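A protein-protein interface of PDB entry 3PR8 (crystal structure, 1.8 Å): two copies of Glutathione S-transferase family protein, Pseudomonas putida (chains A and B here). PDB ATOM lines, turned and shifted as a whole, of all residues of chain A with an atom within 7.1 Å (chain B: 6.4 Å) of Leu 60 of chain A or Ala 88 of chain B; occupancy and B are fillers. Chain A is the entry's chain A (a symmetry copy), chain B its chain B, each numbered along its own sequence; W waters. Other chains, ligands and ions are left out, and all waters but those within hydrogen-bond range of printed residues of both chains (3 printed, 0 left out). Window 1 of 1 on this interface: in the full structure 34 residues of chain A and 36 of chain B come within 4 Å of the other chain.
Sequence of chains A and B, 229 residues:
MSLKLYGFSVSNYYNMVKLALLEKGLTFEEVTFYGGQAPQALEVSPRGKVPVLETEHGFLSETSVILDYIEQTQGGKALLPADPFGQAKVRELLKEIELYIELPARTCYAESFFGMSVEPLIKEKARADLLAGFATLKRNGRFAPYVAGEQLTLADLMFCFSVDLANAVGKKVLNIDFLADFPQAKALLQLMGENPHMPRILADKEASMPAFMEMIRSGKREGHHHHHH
OE2 of Glu 92 of chain B sits at hydrogen-bond distance from OG of Ser 61 of chain A.
The side-chain amino group (NZ) of Lys 89 of chain B is in salt-bridge range of the side-chain carboxylate (OE1) of Glu 92 of chain B, 2.5 Å away.
The backbone NH (N) of Leu 53 of chain A is in hydrogen-bond range of the backbone carbonyl oxygen (O) of Leu 60 of chain A, 2.8 Å away.
The side-chain hydroxyl (OG1) of Thr 55 of chain A lies within hydrogen-bond range of the backbone carbonyl oxygen (O) of Gly 58 of chain A, at 2.9 Å.
Among the printed residues, pairs that only touch across the chains: Val 65 of chain A with Ala 88 of chain B, Thr 55 of chain A with Phe 85 of chain B, Leu 60 of chain A with Ala 88 of chain B, Leu 60 of chain A with Phe 85 of chain B, Phe 59 of chain A with Lys 89 of chain B, Gly 58 of chain A with Phe 85 of chain B, Tyr 69 of chain A with Phe 85 of chain B, Phe 59 of chain A with Phe 85 of chain B, Val 65 of chain A with Arg 91 of chain B, Val 65 of chain A with Glu 92 of chain B, Tyr 69 of chain A with Pro 84 of chain B, Leu 60 of chain A with Glu 92 of chain B and Tyr 69 of chain A with Ala 88 of chain B.
Printed residues of chain B within 4 Å of Leu 60 of chain A: Phe 85 (3.5 Å), Ala 88 (3.5 Å) and Glu 92 (3.8 Å).
Of the printed residues of chain A, Ala 88 of chain B touches Leu 60 (3.5 Å), Val 65 (3.4 Å) and Tyr 69 (3.99 Å).
Of the printed residues of chain B, Tyr 69 of chain A touches Pro 84, Phe 85 and Ala 88.
Of the printed residues of chain A, Lys 89 of chain B touches Phe 59.
Ile 66 of chain A touches none of the printed residues of chain B.
Val 52 of chain A touches none of the printed residues of chain B.
The nearest printed residue of chain A that does not touch Ala 88 of chain B is Ser 61 of chain A (6.2 Å).
The nearest printed residue of chain B that does not touch Val 65 of chain A is Lys 89 of chain B (5.3 Å).
Of the 21 printed residues of chain A, 7 touch a printed residue of chain B.
Along chain A the printed residues that touch a printed residue of chain B span positions 55 to 69.
Hydrophobic or aromatic side chains of chain B within 4 Å of the printed part of chain A: Phe 85 and Ala 88.
Among the printed residues, 14 pairs touch across the chains.
No position is printed for both chains.
Water W2 lies within hydrogen-bond range of OE2 of Glu 92 of chain B (2.6 Å), NZ of Lys 89 of chain B (2.8 Å) and O of Phe 59 of chain A (3.0 Å).
Water W3 lies within hydrogen-bond range of the backbone carbonyl oxygen of Phe 59 of chain A and the side-chain amino group of Lys 89 of chain B.
Water W1 lies within hydrogen-bond range of the side-chain carboxylate of Asp 68 of chain A (2.9 Å) and the guanidinium group of Arg 91 of chain B (3.5 Å).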
ATOM      1  N   LEU A   5      29.216 -15.578  -5.324  1.00  0.00           N
ATOM      2  CA  LEU A   5      30.417 -15.816  -4.523  1.00  0.00           C
ATOM      3  C   LEU A   5      31.591 -15.068  -5.129  1.00  0.00           C
ATOM      4  O   LEU A   5      31.994 -15.352  -6.261  1.00  0.00           O
ATOM      5  CB  LEU A   5      30.734 -17.298  -4.458  1.00  0.00           C
ATOM      6  CG  LEU A   5      31.859 -17.712  -3.512  1.00  0.00           C
ATOM      7  CD1 LEU A   5      31.460 -17.426  -2.054  1.00  0.00           C
ATOM      8  CD2 LEU A   5      32.058 -19.224  -3.760  1.00  0.00           C
ATOM      9  N   VAL A  44      33.819  -3.960  -0.474  1.00  0.00           N
ATOM     10  CA  VAL A  44      33.150  -5.253  -0.644  1.00  0.00           C
ATOM     11  C   VAL A  44      33.428  -6.145   0.555  1.00  0.00           C
ATOM     12  O   VAL A  44      32.530  -6.822   1.064  1.00  0.00           O
ATOM     13  CB  VAL A  44      33.598  -5.949  -1.932  1.00  0.00           C
ATOM     14  CG1 VAL A  44      32.962  -7.328  -2.046  1.00  0.00           C
ATOM     15  CG2 VAL A  44      33.173  -5.088  -3.142  1.00  0.00           C
ATOM     16  N   SER A  45      34.685  -6.140   0.986  1.00  0.00           N
ATOM     17  CA  SER A  45      35.150  -7.020   2.051  1.00  0.00           C
ATOM     18  C   SER A  45      35.971  -6.187   3.038  1.00  0.00           C
ATOM     19  O   SER A  45      37.024  -5.706   2.667  1.00  0.00           O
ATOM     20  CB  SER A  45      36.074  -8.076   1.460  1.00  0.00           C
ATOM     21  OG  SER A  45      36.238  -9.157   2.364  1.00  0.00           O
ATOM     22  N   PRO A  46      35.500  -6.047   4.286  1.00  0.00           N
ATOM     23  CA  PRO A  46      35.992  -5.003   5.194  1.00  0.00           C
ATOM     24  C   PRO A  46      37.435  -5.122   5.660  1.00  0.00           C
ATOM     25  O   PRO A  46      37.978  -4.123   6.107  1.00  0.00           O
ATOM     26  CB  PRO A  46      35.042  -5.084   6.404  1.00  0.00           C
ATOM     27  CG  PRO A  46      33.936  -6.019   6.004  1.00  0.00           C
ATOM     28  CD  PRO A  46      34.426  -6.863   4.878  1.00  0.00           C
ATOM     29  N   PRO A  51      36.709 -15.364   0.715  1.00  0.00           N
ATOM     30  CA  PRO A  51      35.584 -15.068  -0.157  1.00  0.00           C
ATOM     31  C   PRO A  51      34.591 -14.091   0.475  1.00  0.00           C
ATOM     32  O   PRO A  51      34.627 -13.831   1.691  1.00  0.00           O
ATOM     33  CB  PRO A  51      34.927 -16.430  -0.331  1.00  0.00           C
ATOM     34  CG  PRO A  51      35.169 -17.103   1.036  1.00  0.00           C
ATOM     35  CD  PRO A  51      36.525 -16.638   1.442  1.00  0.00           C
ATOM     36  N   VAL A  52      33.705 -13.557  -0.358  1.00  0.00           N
ATOM     37  CA  VAL A  52      32.579 -12.766   0.110  1.00  0.00           C
ATOM     38  C   VAL A  52      31.330 -13.336  -0.545  1.00  0.00           C
ATOM     39  O   VAL A  52      31.362 -13.691  -1.723  1.00  0.00           O
ATOM     40  CB  VAL A  52      32.740 -11.272  -0.259  1.00  0.00           C
ATOM     41  CG1 VAL A  52      31.558 -10.467   0.279  1.00  0.00           C
ATOM     42  CG2 VAL A  52      33.989 -10.721   0.371  1.00  0.00           C
ATOM     43  N   LEU A  53      30.239 -13.427   0.205  1.00  0.00           N
ATOM     44  CA  LEU A  53      28.965 -13.885  -0.347  1.00  0.00           C
ATOM     45  C   LEU A  53      28.059 -12.684  -0.483  1.00  0.00           C
ATOM     46  O   LEU A  53      27.822 -11.980   0.502  1.00  0.00           O
ATOM     47  CB  LEU A  53      28.313 -14.920   0.572  1.00  0.00           C
ATOM     48  CG  LEU A  53      27.005 -15.585   0.061  1.00  0.00           C
ATOM     49  CD1 LEU A  53      27.273 -16.582  -1.078  1.00  0.00           C
ATOM     50  CD2 LEU A  53      26.289 -16.277   1.185  1.00  0.00           C
ATOM     51  N   GLU A  54      27.570 -12.428  -1.700  1.00  0.00           N
ATOM     52  CA  GLU A  54      26.548 -11.397  -1.882  1.00  0.00           C
ATOM     53  C   GLU A  54      25.177 -12.045  -1.816  1.00  0.00           C
ATOM     54  O   GLU A  54      24.898 -13.026  -2.534  1.00  0.00           O
ATOM     55  CB  GLU A  54      26.717 -10.653  -3.221  1.00  0.00           C
ATOM     56  CG  GLU A  54      25.837  -9.384  -3.308  1.00  0.00           C
ATOM     57  CD  GLU A  54      26.068  -8.556  -4.583  1.00  0.00           C
ATOM     58  OE1 GLU A  54      26.595  -9.081  -5.576  1.00  0.00           O
ATOM     59  OE2 GLU A  54      25.715  -7.359  -4.574  1.00  0.00           O
ATOM     60  N   THR A  55      24.342 -11.514  -0.923  1.00  0.00           N
ATOM     61  CA  THR A  55      22.959 -11.965  -0.739  1.00  0.00           C
ATOM     62  C   THR A  55      22.038 -10.795  -1.055  1.00  0.00           C
ATOM     63  O   THR A  55      22.515  -9.685  -1.329  1.00  0.00           O
ATOM     64  CB  THR A  55      22.684 -12.350   0.715  1.00  0.00           C
ATOM     65  OG1 THR A  55      22.638 -11.151   1.514  1.00  0.00           O
ATOM     66  CG2 THR A  55      23.785 -13.284   1.248  1.00  0.00           C
ATOM     67  N   GLY A  58      22.909  -7.942   1.275  1.00  0.00           N
ATOM     68  CA  GLY A  58      24.220  -7.311   1.212  1.00  0.00           C
ATOM     69  C   GLY A  58      25.327  -8.353   1.317  1.00  0.00           C
ATOM     70  O   GLY A  58      25.053  -9.551   1.226  1.00  0.00           O
ATOM     71  N   PHE A  59      26.563  -7.887   1.509  1.00  0.00           N
ATOM     72  CA  PHE A  59      27.741  -8.771   1.527  1.00  0.00           C
ATOM     73  C   PHE A  59      28.019  -9.360   2.908  1.00  0.00           C
ATOM     74  O   PHE A  59      27.878  -8.667   3.940  1.00  0.00           O
ATOM     75  CB  PHE A  59      28.987  -7.992   1.146  1.00  0.00           C
ATOM     76  CG  PHE A  59      29.018  -7.520  -0.288  1.00  0.00           C
ATOM     77  CD1 PHE A  59      29.221  -8.419  -1.326  1.00  0.00           C
ATOM     78  CD2 PHE A  59      28.910  -6.164  -0.584  1.00  0.00           C
ATOM     79  CE1 PHE A  59      29.284  -7.977  -2.634  1.00  0.00           C
ATOM     80  CE2 PHE A  59      28.974  -5.713  -1.903  1.00  0.00           C
ATOM     81  CZ  PHE A  59      29.166  -6.622  -2.921  1.00  0.00           C
ATOM     82  N   LEU A  60      28.483 -10.614   2.919  1.00  0.00           N
ATOM     83  CA  LEU A  60      28.968 -11.257   4.135  1.00  0.00           C
ATOM     84  C   LEU A  60      30.359 -11.797   3.846  1.00  0.00           C
ATOM     85  O   LEU A  60      30.538 -12.470   2.828  1.00  0.00           O
ATOM     86  CB  LEU A  60      28.096 -12.449   4.514  1.00  0.00           C
ATOM     87  CG  LEU A  60      26.911 -12.402   5.458  1.00  0.00           C
ATOM     88  CD1 LEU A  60      26.499 -13.840   5.708  1.00  0.00           C
ATOM     89  CD2 LEU A  60      27.322 -11.696   6.799  1.00  0.00           C
ATOM     90  N   SER A  61      31.324 -11.549   4.739  1.00  0.00           N
ATOM     91  CA  SER A  61      32.682 -12.025   4.554  1.00  0.00           C
ATOM     92  C   SER A  61      32.981 -13.044   5.651  1.00  0.00           C
ATOM     93  O   SER A  61      32.173 -13.225   6.535  1.00  0.00           O
ATOM     94  CB  SER A  61      33.694 -10.857   4.595  1.00  0.00           C
ATOM     95  OG  SER A  61      33.851 -10.367   5.923  1.00  0.00           O
ATOM     96  N   GLU A  62      34.129 -13.719   5.562  1.00  0.00           N
ATOM     97  CA  GLU A  62      34.572 -14.727   6.570  1.00  0.00           C
ATOM     98  C   GLU A  62      33.953 -16.102   6.274  1.00  0.00           C
ATOM     99  O   GLU A  62      32.737 -16.319   6.420  1.00  0.00           O
ATOM    100  CB  GLU A  62      34.291 -14.304   8.025  1.00  0.00           C
ATOM    101  CG  GLU A  62      35.029 -13.032   8.486  1.00  0.00           C
ATOM    102  CD  GLU A  62      36.562 -13.146   8.460  1.00  0.00           C
ATOM    103  OE1 GLU A  62      37.139 -14.256   8.685  1.00  0.00           O
ATOM    104  OE2 GLU A  62      37.195 -12.093   8.233  1.00  0.00           O
ATOM    105  N   THR A  63      34.801 -17.031   5.813  1.00  0.00           N
ATOM    106  CA  THR A  63      34.322 -18.357   5.422  1.00  0.00           C
ATOM    107  C   THR A  63      33.440 -19.011   6.464  1.00  0.00           C
ATOM    108  O   THR A  63      32.360 -19.527   6.152  1.00  0.00           O
ATOM    109  CB  THR A  63      35.534 -19.276   5.070  1.00  0.00           C
ATOM    110  OG1 THR A  63      36.132 -18.771   3.874  1.00  0.00           O
ATOM    111  CG2 THR A  63      35.065 -20.713   4.814  1.00  0.00           C
ATOM    112  N   VAL A  65      31.641 -17.772   8.815  1.00  0.00           N
ATOM    113  CA  VAL A  65      30.379 -17.033   8.908  1.00  0.00           C
ATOM    114  C   VAL A  65      29.497 -17.306   7.683  1.00  0.00           C
ATOM    115  O   VAL A  65      28.295 -17.551   7.826  1.00  0.00           O
ATOM    116  CB  VAL A  65      30.674 -15.521   9.027  1.00  0.00           C
ATOM    117  CG1 VAL A  65      29.373 -14.670   8.907  1.00  0.00           C
ATOM    118  CG2 VAL A  65      31.443 -15.246  10.348  1.00  0.00           C
ATOM    119  N   ILE A  66      30.109 -17.274   6.496  1.00  0.00           N
ATOM    120  CA  ILE A  66      29.403 -17.593   5.248  1.00  0.00           C
ATOM    121  C   ILE A  66      28.793 -19.009   5.290  1.00  0.00           C
ATOM    122  O   ILE A  66      27.615 -19.205   4.952  1.00  0.00           O
ATOM    123  CB  ILE A  66      30.316 -17.410   4.018  1.00  0.00           C
ATOM    124  CG1 ILE A  66      30.623 -15.928   3.797  1.00  0.00           C
ATOM    125  CG2 ILE A  66      29.691 -18.047   2.718  1.00  0.00           C
ATOM    126  CD1 ILE A  66      31.859 -15.673   2.860  1.00  0.00           C
ATOM    127  N   LEU A  67      29.592 -19.992   5.704  1.00  0.00           N
ATOM    128  CA  LEU A  67      29.085 -21.373   5.780  1.00  0.00           C
ATOM    129  C   LEU A  67      27.889 -21.508   6.739  1.00  0.00           C
ATOM    130  O   LEU A  67      26.911 -22.237   6.466  1.00  0.00           O
ATOM    131  CB  LEU A  67      30.222 -22.320   6.208  1.00  0.00           C
ATOM    132  CG  LEU A  67      31.338 -22.481   5.182  1.00  0.00           C
ATOM    133  CD1 LEU A  67      32.521 -23.279   5.797  1.00  0.00           C
ATOM    134  CD2 LEU A  67      30.842 -23.169   3.923  1.00  0.00           C
ATOM    135  N   ASP A  68      27.961 -20.822   7.877  1.00  0.00           N
ATOM    136  CA  ASP A  68      26.851 -20.896   8.822  1.00  0.00           C
ATOM    137  C   ASP A  68      25.602 -20.246   8.230  1.00  0.00           C
ATOM    138  O   ASP A  68      24.467 -20.759   8.383  1.00  0.00           O
ATOM    139  CB  ASP A  68      27.200 -20.197  10.131  1.00  0.00           C
ATOM    140  CG  ASP A  68      27.961 -21.093  11.099  1.00  0.00           C
ATOM    141  OD1 ASP A  68      28.112 -22.327  10.858  1.00  0.00           O
ATOM    142  OD2 ASP A  68      28.450 -20.545  12.104  1.00  0.00           O
ATOM    143  N   TYR A  69      25.796 -19.111   7.577  1.00  0.00           N
ATOM    144  CA  TYR A  69      24.660 -18.456   6.932  1.00  0.00           C
ATOM    145  C   TYR A  69      24.009 -19.366   5.892  1.00  0.00           C
ATOM    146  O   TYR A  69      22.784 -19.540   5.875  1.00  0.00           O
ATOM    147  CB  TYR A  69      25.108 -17.143   6.303  1.00  0.00           C
ATOM    148  CG  TYR A  69      23.983 -16.437   5.596  1.00  0.00           C
ATOM    149  CD1 TYR A  69      23.018 -15.722   6.308  1.00  0.00           C
ATOM    150  CD2 TYR A  69      23.874 -16.512   4.211  1.00  0.00           C
ATOM    151  CE1 TYR A  69      21.976 -15.074   5.641  1.00  0.00           C
ATOM    152  CE2 TYR A  69      22.837 -15.872   3.534  1.00  0.00           C
ATOM    153  CZ  TYR A  69      21.901 -15.149   4.261  1.00  0.00           C
ATOM    154  OH  TYR A  69      20.868 -14.532   3.581  1.00  0.00           O
ATOM    155  N   ILE A  70      24.831 -19.982   5.046  1.00  0.00           N
ATOM    156  CA  ILE A  70      24.316 -20.900   4.018  1.00  0.00           C
ATOM    157  C   ILE A  70      23.560 -22.083   4.634  1.00  0.00           C
ATOM    158  O   ILE A  70      22.485 -22.484   4.164  1.00  0.00           O
ATOM    159  CB  ILE A  70      25.446 -21.379   3.093  1.00  0.00           C
ATOM    160  CG1 ILE A  70      25.923 -20.221   2.224  1.00  0.00           C
ATOM    161  CG2 ILE A  70      24.968 -22.559   2.233  1.00  0.00           C
ATOM    162  CD1 ILE A  70      27.235 -20.485   1.473  1.00  0.00           C
ATOM    163  N   ASP B  83      16.816 -12.417  12.875  1.00  0.00           N
ATOM    164  CA  ASP B  83      16.923 -12.703  11.426  1.00  0.00           C
ATOM    165  C   ASP B  83      18.271 -13.310  11.065  1.00  0.00           C
ATOM    166  O   ASP B  83      19.313 -12.890  11.578  1.00  0.00           O
ATOM    167  CB  ASP B  83      16.646 -11.454  10.567  1.00  0.00           C
ATOM    168  CG  ASP B  83      17.624 -10.312  10.850  1.00  0.00           C
ATOM    169  OD1 ASP B  83      17.615  -9.782  11.982  1.00  0.00           O
ATOM    170  OD2 ASP B  83      18.376  -9.907   9.931  1.00  0.00           O
ATOM    171  N   PRO B  84      18.265 -14.303  10.162  1.00  0.00           N
ATOM    172  CA  PRO B  84      19.545 -14.958   9.945  1.00  0.00           C
ATOM    173  C   PRO B  84      20.663 -14.103   9.329  1.00  0.00           C
ATOM    174  O   PRO B  84      21.837 -14.321   9.660  1.00  0.00           O
ATOM    175  CB  PRO B  84      19.190 -16.168   9.057  1.00  0.00           C
ATOM    176  CG  PRO B  84      17.832 -15.884   8.527  1.00  0.00           C
ATOM    177  CD  PRO B  84      17.144 -15.024   9.524  1.00  0.00           C
ATOM    178  N   PHE B  85      20.350 -13.152   8.452  1.00  0.00           N
ATOM    179  CA  PHE B  85      21.417 -12.283   7.961  1.00  0.00           C
ATOM    180  C   PHE B  85      21.968 -11.393   9.088  1.00  0.00           C
ATOM    181  O   PHE B  85      23.187 -11.197   9.182  1.00  0.00           O
ATOM    182  CB  PHE B  85      20.983 -11.431   6.748  1.00  0.00           C
ATOM    183  CG  PHE B  85      22.135 -10.658   6.102  1.00  0.00           C
ATOM    184  CD1 PHE B  85      22.979 -11.273   5.182  1.00  0.00           C
ATOM    185  CD2 PHE B  85      22.379  -9.331   6.446  1.00  0.00           C
ATOM    186  CE1 PHE B  85      24.058 -10.567   4.606  1.00  0.00           C
ATOM    187  CE2 PHE B  85      23.447  -8.623   5.885  1.00  0.00           C
ATOM    188  CZ  PHE B  85      24.286  -9.238   4.963  1.00  0.00           C
ATOM    189  N   GLY B  86      21.084 -10.831   9.925  1.00  0.00           N
ATOM    190  CA  GLY B  86      21.546 -10.026  11.075  1.00  0.00           C
ATOM    191  C   GLY B  86      22.421 -10.850  12.032  1.00  0.00           C
ATOM    192  O   GLY B  86      23.454 -10.364  12.558  1.00  0.00           O
ATOM    193  N   GLN B  87      22.032 -12.099  12.273  1.00  0.00           N
ATOM    194  CA  GLN B  87      22.885 -12.983  13.084  1.00  0.00           C
ATOM    195  C   GLN B  87      24.253 -13.185  12.460  1.00  0.00           C
ATOM    196  O   GLN B  87      25.268 -13.146  13.180  1.00  0.00           O
ATOM    197  CB  GLN B  87      22.223 -14.343  13.358  1.00  0.00           C
ATOM    198  CG  GLN B  87      20.886 -14.208  14.102  1.00  0.00           C
ATOM    199  CD  GLN B  87      20.275 -15.551  14.418  1.00  0.00           C
ATOM    200  OE1 GLN B  87      20.769 -16.575  13.949  1.00  0.00           O
ATOM    201  NE2 GLN B  87      19.208 -15.565  15.229  1.00  0.00           N
ATOM    202  N   ALA B  88      24.291 -13.404  11.140  1.00  0.00           N
ATOM    203  CA  ALA B  88      25.586 -13.583  10.458  1.00  0.00           C
ATOM    204  C   ALA B  88      26.432 -12.308  10.562  1.00  0.00           C
ATOM    205  O   ALA B  88      27.655 -12.378  10.737  1.00  0.00           O
ATOM    206  CB  ALA B  88      25.392 -13.990   9.005  1.00  0.00           C
ATOM    207  N   LYS B  89      25.799 -11.131  10.479  1.00  0.00           N
ATOM    208  CA  LYS B  89      26.553  -9.893  10.551  1.00  0.00           C
ATOM    209  C   LYS B  89      27.164  -9.741  11.953  1.00  0.00           C
ATOM    210  O   LYS B  89      28.296  -9.284  12.086  1.00  0.00           O
ATOM    211  CB  LYS B  89      25.649  -8.708  10.171  1.00  0.00           C
ATOM    212  CG  LYS B  89      26.347  -7.376  10.111  1.00  0.00           C
ATOM    213  CD  LYS B  89      27.621  -7.408   9.286  1.00  0.00           C
ATOM    214  CE  LYS B  89      27.338  -7.354   7.788  1.00  0.00           C
ATOM    215  NZ  LYS B  89      28.581  -6.993   7.029  1.00  0.00           N
ATOM    216  N   VAL B  90      26.419 -10.140  12.997  1.00  0.00           N
ATOM    217  CA  VAL B  90      26.989 -10.129  14.359  1.00  0.00           C
ATOM    218  C   VAL B  90      28.219 -11.056  14.434  1.00  0.00           C
ATOM    219  O   VAL B  90      29.283 -10.683  14.961  1.00  0.00           O
ATOM    220  CB  VAL B  90      25.957 -10.486  15.453  1.00  0.00           C
ATOM    221  CG1 VAL B  90      26.673 -10.752  16.847  1.00  0.00           C
ATOM    222  CG2 VAL B  90      24.856  -9.387  15.557  1.00  0.00           C
ATOM    223  N   ARG B  91      28.091 -12.253  13.868  1.00  0.00           N
ATOM    224  CA  ARG B  91      29.193 -13.199  13.901  1.00  0.00           C
ATOM    225  C   ARG B  91      30.402 -12.738  13.056  1.00  0.00           C
ATOM    226  O   ARG B  91      31.548 -13.025  13.413  1.00  0.00           O
ATOM    227  CB  ARG B  91      28.691 -14.586  13.489  1.00  0.00           C
ATOM    228  CG  ARG B  91      27.703 -15.145  14.499  1.00  0.00           C
ATOM    229  CD  ARG B  91      26.977 -16.400  14.013  1.00  0.00           C
ATOM    230  NE  ARG B  91      26.256 -17.003  15.137  1.00  0.00           N
ATOM    231  CZ  ARG B  91      24.982 -17.403  15.118  1.00  0.00           C
ATOM    232  NH1 ARG B  91      24.250 -17.298  14.017  1.00  0.00           N
ATOM    233  NH2 ARG B  91      24.443 -17.920  16.225  1.00  0.00           N
ATOM    234  N   GLU B  92      30.147 -12.039  11.949  1.00  0.00           N
ATOM    235  CA  GLU B  92      31.235 -11.457  11.139  1.00  0.00           C
ATOM    236  C   GLU B  92      32.029 -10.426  11.938  1.00  0.00           C
ATOM    237  O   GLU B  92      33.278 -10.419  11.925  1.00  0.00           O
ATOM    238  CB  GLU B  92      30.638 -10.757   9.900  1.00  0.00           C
ATOM    239  CG  GLU B  92      31.670 -10.266   8.904  1.00  0.00           C
ATOM    240  CD  GLU B  92      31.039  -9.332   7.861  1.00  0.00           C
ATOM    241  OE1 GLU B  92      30.184  -8.495   8.224  1.00  0.00           O
ATOM    242  OE2 GLU B  92      31.401  -9.438   6.669  1.00  0.00           O
ATOM    243  N   LEU B  93      31.294  -9.528  12.598  1.00  0.00           N
ATOM    244  CA  LEU B  93      31.901  -8.525  13.453  1.00  0.00           C
ATOM    245  C   LEU B  93      32.679  -9.156  14.604  1.00  0.00           C
ATOM    246  O   LEU B  93      33.782  -8.742  14.883  1.00  0.00           O
ATOM    247  CB  LEU B  93      30.842  -7.526  13.969  1.00  0.00           C
ATOM    248  CG  LEU B  93      30.397  -6.551  12.869  1.00  0.00           C
ATOM    249  CD1 LEU B  93      28.976  -5.957  13.138  1.00  0.00           C
ATOM    250  CD2 LEU B  93      31.445  -5.442  12.771  1.00  0.00           C
HETATM  251  O   HOH W   1      26.642 -20.392  14.368  1.00  0.00           O
HETATM  252  O   HOH W   2      30.470  -7.645   5.110  1.00  0.00           O
HETATM  253  O   HOH W   3      27.026  -6.305   4.748  1.00  0.00           O
